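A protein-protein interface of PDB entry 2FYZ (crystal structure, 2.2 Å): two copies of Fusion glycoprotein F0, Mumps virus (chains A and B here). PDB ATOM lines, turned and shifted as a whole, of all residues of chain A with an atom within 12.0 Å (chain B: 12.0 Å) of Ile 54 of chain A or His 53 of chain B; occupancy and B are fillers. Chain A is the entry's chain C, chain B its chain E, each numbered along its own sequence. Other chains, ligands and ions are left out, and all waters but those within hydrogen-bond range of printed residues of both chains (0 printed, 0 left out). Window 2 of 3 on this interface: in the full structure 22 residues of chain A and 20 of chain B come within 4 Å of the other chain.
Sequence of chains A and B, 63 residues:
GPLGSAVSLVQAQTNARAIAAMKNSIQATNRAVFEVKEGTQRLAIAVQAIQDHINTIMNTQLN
NE2 of Gln 51 of chain A lies close to ND2 of Asn 55 of chain A, at 3.1 Å. O of His 53 of chain B sits at hydrogen-bond distance from N of Met 58 of chain B (3.3 Å).
Among the printed residues, pairs that only touch across the chains: Ala 44 of chain A with Leu 43 of chain B (3.7 Å), Val 47 of chain A with Leu 43 of chain B (3.8 Å), Val 47 of chain A with Val 47 of chain B (3.6 Å), Val 47 of chain A with Ile 50 of chain B (3.5 Å), Gln 51 of chain A with Ile 50 of chain B (3.5 Å), Ile 54 of chain A with Ile 50 of chain B (3.4 Å), Ile 54 of chain A with His 53 of chain B (3.9 Å), Ile 54 of chain A with Ile 54 of chain B (3.6 Å) and Leu 62 of chain A with Leu 62 of chain B (3.4 Å).
Ile 45 of chain A touches none of the printed residues of chain B. Printed residues of chain B within 4 Å of Val 47 of chain A: Leu 43, Val 47 and Ile 50. Gln 51 of chain A touches one residue of chain B. Printed residues of chain B within 4 Å of Ile 54 of chain A: Ile 50, His 53 and Ile 54. No residue of chain B comes within 4 Å of Asn 55 of chain A. No residue of chain B comes within 4 Å of Thr 56 of chain A. No residue of chain B comes within 4 Å of Met 58 of chain A. No residue of chain B comes within 4 Å of Asn 59 of chain A. Printed residues of chain A within 4 Å of Leu 43 of chain B: Ala 44 (3.7 Å) and Val 47 (3.8 Å). No residue of chain A comes within 4 Å of Ala 49 of chain B. Of the printed residues of chain A, Ile 50 of chain B touches Val 47, Gln 51 and Ile 54. No residue of chain A comes within 4 Å of Gln 51 of chain B. Of chain A, only Ile 54 comes within 4 Å of His 53 of chain B. Of chain A, only Ile 54 comes within 4 Å of Ile 54 of chain B. No residue of chain A comes within 4 Å of Thr 56 of chain B. No residue of chain A comes within 4 Å of Ile 57 of chain B. No residue of chain A comes within 4 Å of Met 58 of chain B. Of the printed residues of chain A, Leu 62 of chain B touches Leu 62 (3.4 Å). The nearest residue of chain B that does not touch Ile 54 of chain A is Met 58 of chain B (5.8 Å). The nearest printed residue of chain A that does not touch Val 47 of chain B is Ile 50 of chain A (7.2 Å).
Of the 20 printed residues of chain B, 6 touch a printed residue of chain A. Printed residues of chain B that touch a printed residue of chain A: Leu 43, Val 47, Ile 50, His 53, Ile 54 and Leu 62. Of the 19 printed residues of chain A, 5 touch a printed residue of chain B. Along chain A the printed residues that touch a printed residue of chain B span positions 44 to 62. Among the printed residues, 9 pairs touch across the chains. Among the printed residues, no Asp or Glu carboxylate lies within 4 Å of a Lys or Arg side-chain nitrogen of the other chain.
Val 47 of chain A touches its own counterpart, Val 47 of chain B. Gln 51 of chain A touches Ile 50 of chain B, but with the chains exchanged Ile 50 of chain A does not touch Gln 51 of chain B (7.4 Å). Ile 54 of chain A touches His 53 of chain B, but with the chains exchanged His 53 of chain A does not touch Ile 54 of chain B (8.4 Å). Ile 54 of chain B touches its own counterpart, Ile 54 of chain A.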
ATOM      1  N   ALA A  44     -10.634  19.588   4.309  1.00  0.00           N
ATOM      2  CA  ALA A  44     -10.368  19.899   5.704  1.00  0.00           C
ATOM      3  C   ALA A  44     -11.301  19.064   6.568  1.00  0.00           C
ATOM      4  O   ALA A  44     -10.897  18.530   7.602  1.00  0.00           O
ATOM      5  CB  ALA A  44     -10.605  21.370   5.968  1.00  0.00           C
ATOM      6  N   ILE A  45     -12.555  18.956   6.136  1.00  0.00           N
ATOM      7  CA  ILE A  45     -13.544  18.177   6.865  1.00  0.00           C
ATOM      8  C   ILE A  45     -13.109  16.712   6.937  1.00  0.00           C
ATOM      9  O   ILE A  45     -13.172  16.093   7.994  1.00  0.00           O
ATOM     10  CB  ILE A  45     -14.929  18.287   6.192  1.00  0.00           C
ATOM     11  CG1 ILE A  45     -15.429  19.728   6.299  1.00  0.00           C
ATOM     12  CG2 ILE A  45     -15.917  17.328   6.852  1.00  0.00           C
ATOM     13  CD1 ILE A  45     -16.815  19.952   5.726  1.00  0.00           C
ATOM     14  N   ALA A  46     -12.650  16.165   5.816  1.00  0.00           N
ATOM     15  CA  ALA A  46     -12.202  14.779   5.784  1.00  0.00           C
ATOM     16  C   ALA A  46     -10.986  14.572   6.685  1.00  0.00           C
ATOM     17  O   ALA A  46     -10.865  13.542   7.349  1.00  0.00           O
ATOM     18  CB  ALA A  46     -11.865  14.379   4.363  1.00  0.00           C
ATOM     19  N   VAL A  47     -10.086  15.551   6.708  1.00  0.00           N
ATOM     20  CA  VAL A  47      -8.882  15.449   7.532  1.00  0.00           C
ATOM     21  C   VAL A  47      -9.181  15.408   9.033  1.00  0.00           C
ATOM     22  O   VAL A  47      -8.594  14.613   9.770  1.00  0.00           O
ATOM     23  CB  VAL A  47      -7.914  16.609   7.238  1.00  0.00           C
ATOM     24  CG1 VAL A  47      -6.806  16.665   8.295  1.00  0.00           C
ATOM     25  CG2 VAL A  47      -7.308  16.422   5.856  1.00  0.00           C
ATOM     26  N   GLN A  48     -10.092  16.259   9.487  1.00  0.00           N
ATOM     27  CA  GLN A  48     -10.429  16.275  10.895  1.00  0.00           C
ATOM     28  C   GLN A  48     -11.120  14.961  11.252  1.00  0.00           C
ATOM     29  O   GLN A  48     -10.918  14.423  12.342  1.00  0.00           O
ATOM     30  CB  GLN A  48     -11.331  17.474  11.213  1.00  0.00           C
ATOM     31  CG  GLN A  48     -11.749  17.581  12.684  1.00  0.00           C
ATOM     32  CD  GLN A  48     -10.568  17.648  13.649  1.00  0.00           C
ATOM     33  OE1 GLN A  48      -9.799  18.615  13.658  1.00  0.00           O
ATOM     34  NE2 GLN A  48     -10.425  16.615  14.473  1.00  0.00           N
ATOM     35  N   ALA A  49     -11.918  14.435  10.325  1.00  0.00           N
ATOM     36  CA  ALA A  49     -12.615  13.176  10.566  1.00  0.00           C
ATOM     37  C   ALA A  49     -11.599  12.048  10.699  1.00  0.00           C
ATOM     38  O   ALA A  49     -11.791  11.119  11.482  1.00  0.00           O
ATOM     39  CB  ALA A  49     -13.593  12.880   9.439  1.00  0.00           C
ATOM     40  N   ILE A  50     -10.519  12.119   9.934  1.00  0.00           N
ATOM     41  CA  ILE A  50      -9.491  11.100  10.047  1.00  0.00           C
ATOM     42  C   ILE A  50      -8.798  11.277  11.393  1.00  0.00           C
ATOM     43  O   ILE A  50      -8.466  10.299  12.062  1.00  0.00           O
ATOM     44  CB  ILE A  50      -8.443  11.202   8.925  1.00  0.00           C
ATOM     45  CG1 ILE A  50      -9.038  10.672   7.618  1.00  0.00           C
ATOM     46  CG2 ILE A  50      -7.188  10.421   9.312  1.00  0.00           C
ATOM     47  CD1 ILE A  50      -8.072  10.672   6.450  1.00  0.00           C
ATOM     48  N   GLN A  51      -8.579  12.526  11.792  1.00  0.00           N
ATOM     49  CA  GLN A  51      -7.940  12.791  13.077  1.00  0.00           C
ATOM     50  C   GLN A  51      -8.817  12.262  14.206  1.00  0.00           C
ATOM     51  O   GLN A  51      -8.318  11.682  15.168  1.00  0.00           O
ATOM     52  CB  GLN A  51      -7.707  14.292  13.271  1.00  0.00           C
ATOM     53  CG  GLN A  51      -7.255  14.704  14.679  1.00  0.00           C
ATOM     54  CD  GLN A  51      -5.939  14.061  15.115  1.00  0.00           C
ATOM     55  OE1 GLN A  51      -5.125  13.659  14.286  1.00  0.00           O
ATOM     56  NE2 GLN A  51      -5.724  13.981  16.424  1.00  0.00           N
ATOM     57  N   ASP A  52     -10.124  12.470  14.090  1.00  0.00           N
ATOM     58  CA  ASP A  52     -11.028  11.993  15.120  1.00  0.00           C
ATOM     59  C   ASP A  52     -10.952  10.482  15.239  1.00  0.00           C
ATOM     60  O   ASP A  52     -10.781   9.953  16.331  1.00  0.00           O
ATOM     61  CB  ASP A  52     -12.466  12.414  14.821  1.00  0.00           C
ATOM     62  CG  ASP A  52     -12.651  13.904  14.895  1.00  0.00           C
ATOM     63  OD1 ASP A  52     -11.964  14.545  15.718  1.00  0.00           O
ATOM     64  OD2 ASP A  52     -13.490  14.432  14.142  1.00  0.00           O
ATOM     65  N   HIS A  53     -11.054   9.788  14.110  1.00  0.00           N
ATOM     66  CA  HIS A  53     -11.016   8.332  14.121  1.00  0.00           C
ATOM     67  C   HIS A  53      -9.744   7.778  14.752  1.00  0.00           C
ATOM     68  O   HIS A  53      -9.782   6.770  15.455  1.00  0.00           O
ATOM     69  CB  HIS A  53     -11.176   7.784  12.707  1.00  0.00           C
ATOM     70  CG  HIS A  53     -11.304   6.296  12.659  1.00  0.00           C
ATOM     71  ND1 HIS A  53     -10.287   5.453  13.053  1.00  0.00           N
ATOM     72  CD2 HIS A  53     -12.337   5.496  12.298  1.00  0.00           C
ATOM     73  CE1 HIS A  53     -10.687   4.199  12.938  1.00  0.00           C
ATOM     74  NE2 HIS A  53     -11.927   4.197  12.482  1.00  0.00           N
ATOM     75  N   ILE A  54      -8.621   8.444  14.509  1.00  0.00           N
ATOM     76  CA  ILE A  54      -7.349   8.013  15.076  1.00  0.00           C
ATOM     77  C   ILE A  54      -7.393   8.139  16.598  1.00  0.00           C
ATOM     78  O   ILE A  54      -6.428   7.812  17.295  1.00  0.00           O
ATOM     79  CB  ILE A  54      -6.174   8.861  14.548  1.00  0.00           C
ATOM     80  CG1 ILE A  54      -6.056   8.704  13.035  1.00  0.00           C
ATOM     81  CG2 ILE A  54      -4.867   8.432  15.204  1.00  0.00           C
ATOM     82  CD1 ILE A  54      -4.955   9.554  12.423  1.00  0.00           C
ATOM     83  N   ASN A  55      -8.518   8.621  17.110  1.00  0.00           N
ATOM     84  CA  ASN A  55      -8.722   8.780  18.552  1.00  0.00           C
ATOM     85  C   ASN A  55     -10.001   8.050  18.918  1.00  0.00           C
ATOM     86  O   ASN A  55      -9.990   7.099  19.694  1.00  0.00           O
ATOM     87  CB  ASN A  55      -8.846  10.265  18.909  1.00  0.00           C
ATOM     88  CG  ASN A  55      -7.498  10.928  19.112  1.00  0.00           C
ATOM     89  OD1 ASN A  55      -6.763  10.587  20.040  1.00  0.00           O
ATOM     90  ND2 ASN A  55      -7.163  11.871  18.243  1.00  0.00           N
ATOM     91  N   THR A  56     -11.098   8.518  18.334  1.00  0.00           N
ATOM     92  CA  THR A  56     -12.409   7.944  18.551  1.00  0.00           C
ATOM     93  C   THR A  56     -12.305   6.454  18.853  1.00  0.00           C
ATOM     94  O   THR A  56     -12.773   5.992  19.891  1.00  0.00           O
ATOM     95  CB  THR A  56     -13.298   8.167  17.314  1.00  0.00           C
ATOM     96  OG1 THR A  56     -13.490   9.571  17.113  1.00  0.00           O
ATOM     97  CG2 THR A  56     -14.640   7.501  17.490  1.00  0.00           C
ATOM     98  N   ILE A  57     -11.665   5.709  17.958  1.00  0.00           N
ATOM     99  CA  ILE A  57     -11.513   4.271  18.136  1.00  0.00           C
ATOM    100  C   ILE A  57     -10.063   3.857  18.349  1.00  0.00           C
ATOM    101  O   ILE A  57      -9.764   3.087  19.256  1.00  0.00           O
ATOM    102  CB  ILE A  57     -12.075   3.495  16.916  1.00  0.00           C
ATOM    103  CG1 ILE A  57     -13.493   3.976  16.602  1.00  0.00           C
ATOM    104  CG2 ILE A  57     -12.102   1.996  17.213  1.00  0.00           C
ATOM    105  CD1 ILE A  57     -14.102   3.373  15.350  1.00  0.00           C
ATOM    106  N   MET A  58      -9.169   4.375  17.517  1.00  0.00           N
ATOM    107  CA  MET A  58      -7.756   4.037  17.614  1.00  0.00           C
ATOM    108  C   MET A  58      -7.180   4.283  19.002  1.00  0.00           C
ATOM    109  O   MET A  58      -6.352   3.511  19.483  1.00  0.00           O
ATOM    110  CB  MET A  58      -6.959   4.821  16.567  1.00  0.00           C
ATOM    111  CG  MET A  58      -7.545   4.722  15.171  1.00  0.00           C
ATOM    112  SD  MET A  58      -7.835   3.022  14.666  1.00  0.00           S
ATOM    113  CE  MET A  58      -6.239   2.612  13.970  1.00  0.00           C
ATOM    114  N   ASN A  59      -7.614   5.358  19.648  1.00  0.00           N
ATOM    115  CA  ASN A  59      -7.123   5.678  20.990  1.00  0.00           C
ATOM    116  C   ASN A  59      -7.495   4.570  21.970  1.00  0.00           C
ATOM    117  O   ASN A  59      -6.639   3.825  22.443  1.00  0.00           O
ATOM    118  CB  ASN A  59      -7.722   7.011  21.457  1.00  0.00           C
ATOM    119  CG  ASN A  59      -7.443   7.312  22.923  1.00  0.00           C
ATOM    120  OD1 ASN A  59      -7.939   8.303  23.464  1.00  0.00           O
ATOM    121  ND2 ASN A  59      -6.648   6.465  23.569  1.00  0.00           N
ATOM    122  N   THR A  60      -8.787   4.478  22.263  1.00  0.00           N
ATOM    123  CA  THR A  60      -9.313   3.480  23.176  1.00  0.00           C
ATOM    124  C   THR A  60      -8.990   2.049  22.729  1.00  0.00           C
ATOM    125  O   THR A  60      -8.563   1.227  23.540  1.00  0.00           O
ATOM    126  CB  THR A  60     -10.841   3.625  23.311  1.00  0.00           C
ATOM    127  OG1 THR A  60     -11.160   4.978  23.656  1.00  0.00           O
ATOM    128  CG2 THR A  60     -11.367   2.698  24.390  1.00  0.00           C
ATOM    129  N   GLN A  61      -9.186   1.748  21.446  1.00  0.00           N
ATOM    130  CA  GLN A  61      -8.933   0.398  20.943  1.00  0.00           C
ATOM    131  C   GLN A  61      -7.456   0.089  20.755  1.00  0.00           C
ATOM    132  O   GLN A  61      -7.080  -0.575  19.796  1.00  0.00           O
ATOM    133  CB  GLN A  61      -9.684   0.178  19.643  1.00  0.00           C
ATOM    134  N   LEU A  62      -6.631   0.583  21.680  1.00  0.00           N
ATOM    135  CA  LEU A  62      -5.175   0.382  21.654  1.00  0.00           C
ATOM    136  C   LEU A  62      -4.422   1.228  22.700  1.00  0.00           C
ATOM    137  O   LEU A  62      -3.624   2.103  22.296  1.00  0.00           O
ATOM    138  CB  LEU A  62      -4.622   0.691  20.258  1.00  0.00           C
ATOM    139  CG  LEU A  62      -4.551  -0.436  19.219  1.00  0.00           C
ATOM    140  CD1 LEU A  62      -3.820   0.049  17.987  1.00  0.00           C
ATOM    141  CD2 LEU A  62      -3.844  -1.637  19.808  1.00  0.00           C
ATOM    142  N   LEU B  43      -3.329  22.831   5.630  1.00  0.00           N
ATOM    143  CA  LEU B  43      -3.967  21.528   5.650  1.00  0.00           C
ATOM    144  C   LEU B  43      -2.909  20.452   5.415  1.00  0.00           C
ATOM    145  O   LEU B  43      -2.924  19.405   6.059  1.00  0.00           O
ATOM    146  CB  LEU B  43      -5.063  21.462   4.579  1.00  0.00           C
ATOM    147  CG  LEU B  43      -6.039  20.285   4.656  1.00  0.00           C
ATOM    148  CD1 LEU B  43      -6.640  20.181   6.053  1.00  0.00           C
ATOM    149  CD2 LEU B  43      -7.134  20.476   3.624  1.00  0.00           C
ATOM    150  N   ALA B  44      -1.978  20.720   4.503  1.00  0.00           N
ATOM    151  CA  ALA B  44      -0.923  19.766   4.198  1.00  0.00           C
ATOM    152  C   ALA B  44      -0.074  19.528   5.443  1.00  0.00           C
ATOM    153  O   ALA B  44       0.295  18.394   5.754  1.00  0.00           O
ATOM    154  CB  ALA B  44      -0.064  20.286   3.059  1.00  0.00           C
ATOM    155  N   ILE B  45       0.233  20.602   6.157  1.00  0.00           N
ATOM    156  CA  ILE B  45       1.014  20.491   7.374  1.00  0.00           C
ATOM    157  C   ILE B  45       0.250  19.643   8.391  1.00  0.00           C
ATOM    158  O   ILE B  45       0.840  18.807   9.079  1.00  0.00           O
ATOM    159  CB  ILE B  45       1.323  21.889   7.942  1.00  0.00           C
ATOM    160  CG1 ILE B  45       2.473  22.505   7.145  1.00  0.00           C
ATOM    161  CG2 ILE B  45       1.690  21.806   9.418  1.00  0.00           C
ATOM    162  CD1 ILE B  45       2.635  23.999   7.358  1.00  0.00           C
ATOM    163  N   ALA B  46      -1.065  19.838   8.466  1.00  0.00           N
ATOM    164  CA  ALA B  46      -1.895  19.079   9.391  1.00  0.00           C
ATOM    165  C   ALA B  46      -1.893  17.611   8.987  1.00  0.00           C
ATOM    166  O   ALA B  46      -1.804  16.714   9.830  1.00  0.00           O
ATOM    167  CB  ALA B  46      -3.315  19.619   9.380  1.00  0.00           C
ATOM    168  N   VAL B  47      -1.997  17.374   7.687  1.00  0.00           N
ATOM    169  CA  VAL B  47      -1.997  16.021   7.154  1.00  0.00           C
ATOM    170  C   VAL B  47      -0.664  15.326   7.422  1.00  0.00           C
ATOM    171  O   VAL B  47      -0.622  14.130   7.720  1.00  0.00           O
ATOM    172  CB  VAL B  47      -2.293  16.050   5.647  1.00  0.00           C
ATOM    173  CG1 VAL B  47      -1.932  14.724   5.001  1.00  0.00           C
ATOM    174  CG2 VAL B  47      -3.764  16.374   5.442  1.00  0.00           C
ATOM    175  N   GLN B  48       0.424  16.080   7.322  1.00  0.00           N
ATOM    176  CA  GLN B  48       1.750  15.532   7.569  1.00  0.00           C
ATOM    177  C   GLN B  48       1.892  15.142   9.039  1.00  0.00           C
ATOM    178  O   GLN B  48       2.589  14.181   9.369  1.00  0.00           O
ATOM    179  CB  GLN B  48       2.822  16.559   7.205  1.00  0.00           C
ATOM    180  CG  GLN B  48       4.221  16.196   7.677  1.00  0.00           C
ATOM    181  CD  GLN B  48       4.775  14.978   6.975  1.00  0.00           C
ATOM    182  OE1 GLN B  48       4.155  14.436   6.069  1.00  0.00           O
ATOM    183  NE2 GLN B  48       5.957  14.542   7.390  1.00  0.00           N
ATOM    184  N   ALA B  49       1.230  15.885   9.921  1.00  0.00           N
ATOM    185  CA  ALA B  49       1.302  15.584  11.349  1.00  0.00           C
ATOM    186  C   ALA B  49       0.463  14.342  11.683  1.00  0.00           C
ATOM    187  O   ALA B  49       0.818  13.555  12.562  1.00  0.00           O
ATOM    188  CB  ALA B  49       0.834  16.789  12.170  1.00  0.00           C
ATOM    189  N   ILE B  50      -0.647  14.171  10.974  1.00  0.00           N
ATOM    190  CA  ILE B  50      -1.510  13.017  11.185  1.00  0.00           C
ATOM    191  C   ILE B  50      -0.794  11.771  10.669  1.00  0.00           C
ATOM    192  O   ILE B  50      -0.992  10.665  11.175  1.00  0.00           O
ATOM    193  CB  ILE B  50      -2.854  13.205  10.454  1.00  0.00           C
ATOM    194  CG1 ILE B  50      -3.671  14.275  11.186  1.00  0.00           C
ATOM    195  CG2 ILE B  50      -3.605  11.875  10.360  1.00  0.00           C
ATOM    196  CD1 ILE B  50      -4.925  14.723  10.462  1.00  0.00           C
ATOM    197  N   GLN B  51       0.054  11.964   9.665  1.00  0.00           N
ATOM    198  CA  GLN B  51       0.819  10.868   9.096  1.00  0.00           C
ATOM    199  C   GLN B  51       1.879  10.407  10.096  1.00  0.00           C
ATOM    200  O   GLN B  51       2.006   9.214  10.367  1.00  0.00           O
ATOM    201  CB  GLN B  51       1.491  11.314   7.792  1.00  0.00           C
ATOM    202  CG  GLN B  51       2.422  10.282   7.160  1.00  0.00           C
ATOM    203  CD  GLN B  51       1.718   8.986   6.787  1.00  0.00           C
ATOM    204  OE1 GLN B  51       0.490   8.922   6.741  1.00  0.00           O
ATOM    205  NE2 GLN B  51       2.498   7.950   6.502  1.00  0.00           N
ATOM    206  N   ASP B  52       2.637  11.354  10.644  1.00  0.00           N
ATOM    207  CA  ASP B  52       3.678  11.020  11.610  1.00  0.00           C
ATOM    208  C   ASP B  52       3.086  10.233  12.769  1.00  0.00           C
ATOM    209  O   ASP B  52       3.658   9.242  13.221  1.00  0.00           O
ATOM    210  CB  ASP B  52       4.346  12.283  12.162  1.00  0.00           C
ATOM    211  CG  ASP B  52       5.051  13.091  11.090  1.00  0.00           C
ATOM    212  OD1 ASP B  52       5.664  12.485  10.187  1.00  0.00           O
ATOM    213  OD2 ASP B  52       5.006  14.339  11.163  1.00  0.00           O
ATOM    214  N   HIS B  53       1.933  10.685  13.243  1.00  0.00           N
ATOM    215  CA  HIS B  53       1.249  10.043  14.356  1.00  0.00           C
ATOM    216  C   HIS B  53       0.929   8.586  14.046  1.00  0.00           C
ATOM    217  O   HIS B  53       1.189   7.693  14.851  1.00  0.00           O
ATOM    218  CB  HIS B  53      -0.042  10.803  14.667  1.00  0.00           C
ATOM    219  CG  HIS B  53      -0.725  10.361  15.921  1.00  0.00           C
ATOM    220  ND1 HIS B  53      -1.909  10.917  16.357  1.00  0.00           N
ATOM    221  CD2 HIS B  53      -0.391   9.423  16.842  1.00  0.00           C
ATOM    222  CE1 HIS B  53      -2.274  10.342  17.489  1.00  0.00           C
ATOM    223  NE2 HIS B  53      -1.369   9.431  17.804  1.00  0.00           N
ATOM    224  N   ILE B  54       0.360   8.357  12.868  1.00  0.00           N
ATOM    225  CA  ILE B  54      -0.018   7.019  12.439  1.00  0.00           C
ATOM    226  C   ILE B  54       1.160   6.054  12.349  1.00  0.00           C
ATOM    227  O   ILE B  54       1.015   4.865  12.626  1.00  0.00           O
ATOM    228  CB  ILE B  54      -0.728   7.073  11.075  1.00  0.00           C
ATOM    229  CG1 ILE B  54      -2.074   7.781  11.230  1.00  0.00           C
ATOM    230  CG2 ILE B  54      -0.910   5.671  10.516  1.00  0.00           C
ATOM    231  CD1 ILE B  54      -2.821   7.951   9.930  1.00  0.00           C
ATOM    232  N   ASN B  55       2.327   6.558  11.964  1.00  0.00           N
ATOM    233  CA  ASN B  55       3.492   5.697  11.847  1.00  0.00           C
ATOM    234  C   ASN B  55       4.384   5.708  13.075  1.00  0.00           C
ATOM    235  O   ASN B  55       5.481   5.150  13.057  1.00  0.00           O
ATOM    236  CB  ASN B  55       4.309   6.073  10.615  1.00  0.00           C
ATOM    237  CG  ASN B  55       3.619   5.686   9.326  1.00  0.00           C
ATOM    238  OD1 ASN B  55       3.172   4.547   9.167  1.00  0.00           O
ATOM    239  ND2 ASN B  55       3.533   6.629   8.396  1.00  0.00           N
ATOM    240  N   THR B  56       3.920   6.342  14.144  1.00  0.00           N
ATOM    241  CA  THR B  56       4.698   6.392  15.373  1.00  0.00           C
ATOM    242  C   THR B  56       3.880   5.821  16.521  1.00  0.00           C
ATOM    243  O   THR B  56       3.906   4.617  16.778  1.00  0.00           O
ATOM    244  CB  THR B  56       5.114   7.834  15.725  1.00  0.00           C
ATOM    245  OG1 THR B  56       5.878   8.389  14.647  1.00  0.00           O
ATOM    246  CG2 THR B  56       5.962   7.849  16.990  1.00  0.00           C
ATOM    247  N   ILE B  57       3.146   6.696  17.198  1.00  0.00           N
ATOM    248  CA  ILE B  57       2.312   6.302  18.328  1.00  0.00           C
ATOM    249  C   ILE B  57       1.329   5.193  17.944  1.00  0.00           C
ATOM    250  O   ILE B  57       0.673   4.608  18.807  1.00  0.00           O
ATOM    251  CB  ILE B  57       1.524   7.518  18.874  1.00  0.00           C
ATOM    252  CG1 ILE B  57       2.472   8.707  19.060  1.00  0.00           C
ATOM    253  CG2 ILE B  57       0.869   7.165  20.206  1.00  0.00           C
ATOM    254  CD1 ILE B  57       1.785   9.982  19.503  1.00  0.00           C
ATOM    255  N   MET B  58       1.231   4.907  16.648  1.00  0.00           N
ATOM    256  CA  MET B  58       0.335   3.867  16.164  1.00  0.00           C
ATOM    257  C   MET B  58       1.130   2.739  15.516  1.00  0.00           C
ATOM    258  O   MET B  58       0.578   1.690  15.179  1.00  0.00           O
ATOM    259  CB  MET B  58      -0.655   4.455  15.172  1.00  0.00           C
ATOM    260  N   ASN B  59       2.429   2.962  15.339  1.00  0.00           N
ATOM    261  CA  ASN B  59       3.313   1.959  14.748  1.00  0.00           C
ATOM    262  C   ASN B  59       3.979   1.129  15.835  1.00  0.00           C
ATOM    263  O   ASN B  59       3.737  -0.073  15.953  1.00  0.00           O
ATOM    264  CB  ASN B  59       4.398   2.626  13.902  1.00  0.00           C
ATOM    265  CG  ASN B  59       5.661   1.788  13.806  1.00  0.00           C
ATOM    266  OD1 ASN B  59       5.613   0.611  13.452  1.00  0.00           O
ATOM    267  ND2 ASN B  59       6.799   2.391  14.126  1.00  0.00           N
ATOM    268  N   THR B  60       4.830   1.780  16.620  1.00  0.00           N
ATOM    269  CA  THR B  60       5.536   1.113  17.706  1.00  0.00           C
ATOM    270  C   THR B  60       4.526   0.584  18.720  1.00  0.00           C
ATOM    271  O   THR B  60       4.779  -0.411  19.401  1.00  0.00           O
ATOM    272  CB  THR B  60       6.507   2.082  18.417  1.00  0.00           C
ATOM    273  OG1 THR B  60       7.399   2.656  17.455  1.00  0.00           O
ATOM    274  CG2 THR B  60       7.322   1.344  19.474  1.00  0.00           C
ATOM    275  N   GLN B  61       3.380   1.252  18.809  1.00  0.00           N
ATOM    276  CA  GLN B  61       2.326   0.848  19.732  1.00  0.00           C
ATOM    277  C   GLN B  61       1.803  -0.538  19.365  1.00  0.00           C
ATOM    278  O   GLN B  61       0.989  -1.118  20.086  1.00  0.00           O
ATOM    279  CB  GLN B  61       1.188   1.860  19.705  1.00  0.00           C
ATOM    280  N   LEU B  62       2.276  -1.062  18.238  1.00  0.00           N
ATOM    281  CA  LEU B  62       1.870  -2.380  17.767  1.00  0.00           C
ATOM    282  C   LEU B  62       3.099  -3.226  17.438  1.00  0.00           C
ATOM    283  O   LEU B  62       3.264  -3.594  16.256  1.00  0.00           O
ATOM    284  CB  LEU B  62       0.974  -2.244  16.530  1.00  0.00           C
ATOM    285  CG  LEU B  62      -0.359  -1.521  16.752  1.00  0.00           C
ATOM    286  CD1 LEU B  62      -1.057  -1.290  15.423  1.00  0.00           C
ATOM    287  CD2 LEU B  62      -1.236  -2.343  17.683  1.00  0.00           C
